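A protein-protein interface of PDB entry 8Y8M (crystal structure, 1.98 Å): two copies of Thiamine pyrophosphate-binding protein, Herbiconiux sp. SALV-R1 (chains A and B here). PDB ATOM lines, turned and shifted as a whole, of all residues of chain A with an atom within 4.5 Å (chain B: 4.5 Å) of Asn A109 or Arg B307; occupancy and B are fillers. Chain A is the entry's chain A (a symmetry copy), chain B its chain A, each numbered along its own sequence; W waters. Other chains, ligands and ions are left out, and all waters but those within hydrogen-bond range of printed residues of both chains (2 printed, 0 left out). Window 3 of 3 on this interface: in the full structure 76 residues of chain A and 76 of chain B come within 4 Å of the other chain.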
ATOM      1  N   GLU A 107     -21.851  24.648   1.294  1.00  0.00           N
ATOM      2  CA  GLU A 107     -20.459  24.518   1.764  1.00  0.00           C
ATOM      3  C   GLU A 107     -20.226  25.176   3.128  1.00  0.00           C
ATOM      4  O   GLU A 107     -19.168  25.766   3.380  1.00  0.00           O
ATOM      5  CB  GLU A 107     -19.485  25.094   0.697  1.00  0.00           C
ATOM      6  CG  GLU A 107     -19.374  24.249  -0.529  1.00  0.00           C
ATOM      7  CD  GLU A 107     -18.672  22.919  -0.256  1.00  0.00           C
ATOM      8  OE1 GLU A 107     -17.619  22.926   0.410  1.00  0.00           O
ATOM      9  OE2 GLU A 107     -19.082  21.885  -0.791  1.00  0.00           O
ATOM     10  N   THR A 108     -21.178  25.044   4.065  1.00  0.00           N
ATOM     11  CA  THR A 108     -20.912  25.552   5.405  1.00  0.00           C
ATOM     12  C   THR A 108     -20.762  24.438   6.441  1.00  0.00           C
ATOM     13  O   THR A 108     -20.920  24.703   7.629  1.00  0.00           O
ATOM     14  CB  THR A 108     -21.997  26.521   5.871  1.00  0.00           C
ATOM     15  OG1 THR A 108     -23.260  25.869   5.811  1.00  0.00           O
ATOM     16  CG2 THR A 108     -22.007  27.742   4.876  1.00  0.00           C
ATOM     17  N   ASN A 109     -20.491  23.197   6.019  1.00  0.00           N
ATOM     18  CA  ASN A 109     -20.344  22.068   6.938  1.00  0.00           C
ATOM     19  C   ASN A 109     -21.564  21.936   7.876  1.00  0.00           C
ATOM     20  O   ASN A 109     -21.438  21.743   9.086  1.00  0.00           O
ATOM     21  CB  ASN A 109     -19.044  22.184   7.742  1.00  0.00           C
ATOM     22  CG  ASN A 109     -17.778  21.911   6.934  1.00  0.00           C
ATOM     23  OD1 ASN A 109     -17.768  21.144   5.976  1.00  0.00           O
ATOM     24  ND2 ASN A 109     -16.673  22.447   7.411  1.00  0.00           N
ATOM     25  N   THR A 110     -22.759  22.055   7.303  1.00  0.00           N
ATOM     26  CA  THR A 110     -23.983  22.145   8.063  1.00  0.00           C
ATOM     27  C   THR A 110     -24.763  20.832   8.101  1.00  0.00           C
ATOM     28  O   THR A 110     -24.338  19.783   7.614  1.00  0.00           O
ATOM     29  CB  THR A 110     -24.853  23.314   7.559  1.00  0.00           C
ATOM     30  OG1 THR A 110     -25.780  23.666   8.613  1.00  0.00           O
ATOM     31  CG2 THR A 110     -25.552  23.017   6.240  1.00  0.00           C
ATOM     32  N   ARG B 276     -13.240  22.008  12.289  1.00  0.00           N
ATOM     33  CA  ARG B 276     -13.758  22.851  11.227  1.00  0.00           C
ATOM     34  C   ARG B 276     -14.840  23.797  11.731  1.00  0.00           C
ATOM     35  O   ARG B 276     -15.586  23.481  12.656  1.00  0.00           O
ATOM     36  CB  ARG B 276     -14.346  21.983  10.128  1.00  0.00           C
ATOM     37  CG  ARG B 276     -13.374  20.923   9.697  1.00  0.00           C
ATOM     38  CD  ARG B 276     -14.101  19.907   8.851  1.00  0.00           C
ATOM     39  NE  ARG B 276     -14.628  18.805   9.655  1.00  0.00           N
ATOM     40  CZ  ARG B 276     -15.142  17.702   9.128  1.00  0.00           C
ATOM     41  NH1 ARG B 276     -15.387  17.608   7.827  1.00  0.00           N
ATOM     42  NH2 ARG B 276     -15.411  16.671   9.918  1.00  0.00           N
ATOM     43  N   PHE B 277     -14.945  24.946  11.078  1.00  0.00           N
ATOM     44  CA  PHE B 277     -16.156  25.746  11.165  1.00  0.00           C
ATOM     45  C   PHE B 277     -17.300  24.940  10.546  1.00  0.00           C
ATOM     46  O   PHE B 277     -17.132  24.336   9.478  1.00  0.00           O
ATOM     47  CB  PHE B 277     -15.936  27.049  10.412  1.00  0.00           C
ATOM     48  CG  PHE B 277     -14.896  27.938  11.056  1.00  0.00           C
ATOM     49  CD1 PHE B 277     -15.089  28.474  12.345  1.00  0.00           C
ATOM     50  CD2 PHE B 277     -13.665  28.177  10.383  1.00  0.00           C
ATOM     51  CE1 PHE B 277     -14.103  29.309  12.952  1.00  0.00           C
ATOM     52  CE2 PHE B 277     -12.650  29.009  10.972  1.00  0.00           C
ATOM     53  CZ  PHE B 277     -12.878  29.542  12.299  1.00  0.00           C
ATOM     54  N   GLY B 278     -18.450  24.907  11.220  1.00  0.00           N
ATOM     55  CA  GLY B 278     -19.558  24.075  10.781  1.00  0.00           C
ATOM     56  C   GLY B 278     -20.627  23.997  11.860  1.00  0.00           C
ATOM     57  O   GLY B 278     -20.726  24.875  12.739  1.00  0.00           O
ATOM     58  N   LEU B 279     -21.432  22.933  11.773  1.00  0.00           N
ATOM     59  CA  LEU B 279     -22.540  22.781  12.712  1.00  0.00           C
ATOM     60  C   LEU B 279     -22.079  22.888  14.172  1.00  0.00           C
ATOM     61  O   LEU B 279     -22.720  23.578  14.973  1.00  0.00           O
ATOM     62  CB  LEU B 279     -23.250  21.442  12.454  1.00  0.00           C
ATOM     63  CG  LEU B 279     -24.490  21.170  13.289  1.00  0.00           C
ATOM     64  CD1 LEU B 279     -25.584  22.174  12.920  1.00  0.00           C
ATOM     65  CD2 LEU B 279     -24.939  19.777  12.959  1.00  0.00           C
ATOM     66  N   ARG B 303      -8.804  23.730   2.518  1.00  0.00           N
ATOM     67  CA  ARG B 303     -10.149  24.261   2.274  1.00  0.00           C
ATOM     68  C   ARG B 303     -10.859  24.668   3.569  1.00  0.00           C
ATOM     69  O   ARG B 303     -11.739  25.538   3.548  1.00  0.00           O
ATOM     70  CB  ARG B 303     -11.034  23.249   1.571  1.00  0.00           C
ATOM     71  CG  ARG B 303     -11.514  22.094   2.499  1.00  0.00           C
ATOM     72  CD  ARG B 303     -12.554  21.276   1.751  1.00  0.00           C
ATOM     73  NE  ARG B 303     -11.907  20.298   0.874  1.00  0.00           N
ATOM     74  CZ  ARG B 303     -12.387  19.976  -0.327  1.00  0.00           C
ATOM     75  NH1 ARG B 303     -13.632  20.279  -0.676  1.00  0.00           N
ATOM     76  NH2 ARG B 303     -11.634  19.283  -1.170  1.00  0.00           N
ATOM     77  N   GLU B 304     -10.467  24.097   4.697  1.00  0.00           N
ATOM     78  CA  GLU B 304     -11.138  24.431   5.953  1.00  0.00           C
ATOM     79  C   GLU B 304     -10.656  25.752   6.556  1.00  0.00           C
ATOM     80  O   GLU B 304     -11.384  26.344   7.360  1.00  0.00           O
ATOM     81  CB  GLU B 304     -10.903  23.298   6.950  1.00  0.00           C
ATOM     82  CG  GLU B 304     -11.476  21.917   6.570  1.00  0.00           C
ATOM     83  CD  GLU B 304     -12.962  21.932   6.135  1.00  0.00           C
ATOM     84  OE1 GLU B 304     -13.778  22.777   6.643  1.00  0.00           O
ATOM     85  OE2 GLU B 304     -13.345  20.994   5.390  1.00  0.00           O
ATOM     86  N   LEU B 305      -9.471  26.255   6.179  1.00  0.00           N
ATOM     87  CA  LEU B 305      -8.933  27.433   6.883  1.00  0.00           C
ATOM     88  C   LEU B 305      -9.718  28.680   6.570  1.00  0.00           C
ATOM     89  O   LEU B 305      -9.800  29.115   5.408  1.00  0.00           O
ATOM     90  CB  LEU B 305      -7.450  27.679   6.597  1.00  0.00           C
ATOM     91  CG  LEU B 305      -6.555  26.459   6.602  1.00  0.00           C
ATOM     92  CD1 LEU B 305      -5.053  26.813   6.254  1.00  0.00           C
ATOM     93  CD2 LEU B 305      -6.625  25.960   8.026  1.00  0.00           C
ATOM     94  N   GLY B 306     -10.231  29.298   7.617  1.00  0.00           N
ATOM     95  CA  GLY B 306     -10.967  30.528   7.405  1.00  0.00           C
ATOM     96  C   GLY B 306     -12.268  30.318   6.670  1.00  0.00           C
ATOM     97  O   GLY B 306     -12.801  31.274   6.102  1.00  0.00           O
ATOM     98  N   ARG B 307     -12.806  29.086   6.659  1.00  0.00           N
ATOM     99  CA  ARG B 307     -13.919  28.784   5.753  1.00  0.00           C
ATOM    100  C   ARG B 307     -15.105  29.717   5.996  1.00  0.00           C
ATOM    101  O   ARG B 307     -15.629  30.317   5.048  1.00  0.00           O
ATOM    102  CB  ARG B 307     -14.337  27.312   5.888  1.00  0.00           C
ATOM    103  CG  ARG B 307     -15.539  26.910   4.984  1.00  0.00           C
ATOM    104  CD  ARG B 307     -16.176  25.523   5.375  1.00  0.00           C
ATOM    105  NE  ARG B 307     -15.446  24.364   4.860  1.00  0.00           N
ATOM    106  CZ  ARG B 307     -15.836  23.658   3.797  1.00  0.00           C
ATOM    107  NH1 ARG B 307     -16.814  24.082   3.011  1.00  0.00           N
ATOM    108  NH2 ARG B 307     -15.208  22.522   3.502  1.00  0.00           N
ATOM    109  N   LEU B 308     -15.533  29.863   7.253  1.00  0.00           N
ATOM    110  CA  LEU B 308     -16.772  30.646   7.509  1.00  0.00           C
ATOM    111  C   LEU B 308     -16.497  31.964   8.255  1.00  0.00           C
ATOM    112  O   LEU B 308     -17.386  32.837   8.242  1.00  0.00           O
ATOM    113  CB  LEU B 308     -17.735  29.751   8.283  1.00  0.00           C
ATOM    114  CG  LEU B 308     -18.164  28.464   7.574  1.00  0.00           C
ATOM    115  CD1 LEU B 308     -19.085  27.632   8.445  1.00  0.00           C
ATOM    116  CD2 LEU B 308     -18.827  28.788   6.249  1.00  0.00           C
ATOM    117  N   GLN B 309     -15.351  32.081   8.920  1.00  0.00           N
ATOM    118  CA  GLN B 309     -15.007  33.352   9.615  1.00  0.00           C
ATOM    119  C   GLN B 309     -13.501  33.644   9.471  1.00  0.00           C
ATOM    120  O   GLN B 309     -12.732  32.703   9.203  1.00  0.00           O
ATOM    121  CB  GLN B 309     -15.562  33.342  11.042  1.00  0.00           C
ATOM    122  CG  GLN B 309     -14.751  32.565  12.067  1.00  0.00           C
ATOM    123  CD  GLN B 309     -15.463  32.481  13.398  1.00  0.00           C
ATOM    124  OE1 GLN B 309     -16.422  31.720  13.567  1.00  0.00           O
ATOM    125  NE2 GLN B 309     -15.012  33.279  14.353  1.00  0.00           N
ATOM    126  N   TYR B 415     -21.912  15.723  10.969  1.00  0.00           N
ATOM    127  CA  TYR B 415     -22.738  16.521  10.070  1.00  0.00           C
ATOM    128  C   TYR B 415     -23.829  15.713   9.380  1.00  0.00           C
ATOM    129  O   TYR B 415     -24.884  16.272   9.046  1.00  0.00           O
ATOM    130  CB  TYR B 415     -21.857  17.185   9.022  1.00  0.00           C
ATOM    131  CG  TYR B 415     -20.725  18.036   9.555  1.00  0.00           C
ATOM    132  CD1 TYR B 415     -20.809  18.685  10.775  1.00  0.00           C
ATOM    133  CD2 TYR B 415     -19.538  18.129   8.838  1.00  0.00           C
ATOM    134  CE1 TYR B 415     -19.762  19.451  11.245  1.00  0.00           C
ATOM    135  CE2 TYR B 415     -18.492  18.878   9.285  1.00  0.00           C
ATOM    136  CZ  TYR B 415     -18.602  19.550  10.486  1.00  0.00           C
ATOM    137  OH  TYR B 415     -17.530  20.318  10.908  1.00  0.00           O
HETATM  138  O   HOH W   1     -15.498  19.606   5.686  1.00  0.00           O
HETATM  139  O   HOH W   2     -15.903  20.843   1.303  1.00  0.00           O
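NE of Arg B307 is in salt-bridge range of OE1 of Glu B304, at 2.9 Å.
Of chain B, only Arg B276, Phe B277, Gly B278, Leu B279, Glu B304, Arg B307 and Tyr B415 come within 4 Å of Asn A109.
Of the printed residues of chain A, Arg B307 touches Glu A107 (2.9 Å) and Asn A109 (3.4 Å).
Of the printed residues of chain B, Glu A107 touches Arg B307 (2.9 Å).
Of the printed residues of chain A, Gly B278 touches Thr A108 and Asn A109.
Of the printed residues of chain A, Tyr B415 touches Asn A109 (3.5 Å) and Thr A110 (3.8 Å).
Printed residues of chain A within 4 Å of Phe B277: Asn A109 (2.8 Å).
The nearest printed residue of chain B that does not touch Asn A109 is Leu B308 (5.2 Å).
The nearest printed residue of chain A that does not touch Arg B307 is Thr A108 (4.6 Å).
Water W1 lies within hydrogen-bond range of OE2 of Glu B304, OD1 of Asn A109 and NH1 of Arg B276.
Water W2 lies within hydrogen-bond range of OE1 of Glu A107, NH2 of Arg B307 and NH1 of Arg B303.
O of Thr A108 touches CA of Gly B278 (3.5 Å).
Leu B308 touches Thr A108 (CD1 to O, 3.6 Å).
ND2 of Asn A109 touches CB of Arg B276, 3.6 Å away.
Asn A109 touches Gly B278.
Asn A109 touches Tyr B415 (O to CD1, 3.5 Å).
Tyr B415 touches Thr A110 (O to O, 3.8 Å).
The backbone carbonyl oxygen (O) of Phe B277 sits at hydrogen-bond distance from the side-chain amide nitrogen (ND2) of Asn A109 (2.8 Å).
O of Asn A109 sits at hydrogen-bond distance from N of Leu B279 (2.9 Å).
OE1 of Glu B304 lies within hydrogen-bond range of ND2 of Asn A109, at 3.0 Å.
The side-chain carboxylate of Glu A107 lies within salt-bridge range of the guanidinium group of Arg B307, at 3.0 Å.
NE of Arg B307 sits close to ND2 of Asn A109.
No position is printed for both chains.
Of the 11 pairs that touch across the chains among the printed residues, none has its exchanged pair printed and touching as well.
Of the 4 printed residues of chain A, 4 touch a printed residue of chain B.
Along chain B the printed residues that touch a printed residue of chain A span positions 276 to 415.
Among the printed residues, 11 pairs touch across the chains.
Among the printed residues, Asp or Glu carboxylates within 4 Å of a Lys or Arg side-chain nitrogen of the other chain: Glu A107 with Arg B307 (3.0 Å).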
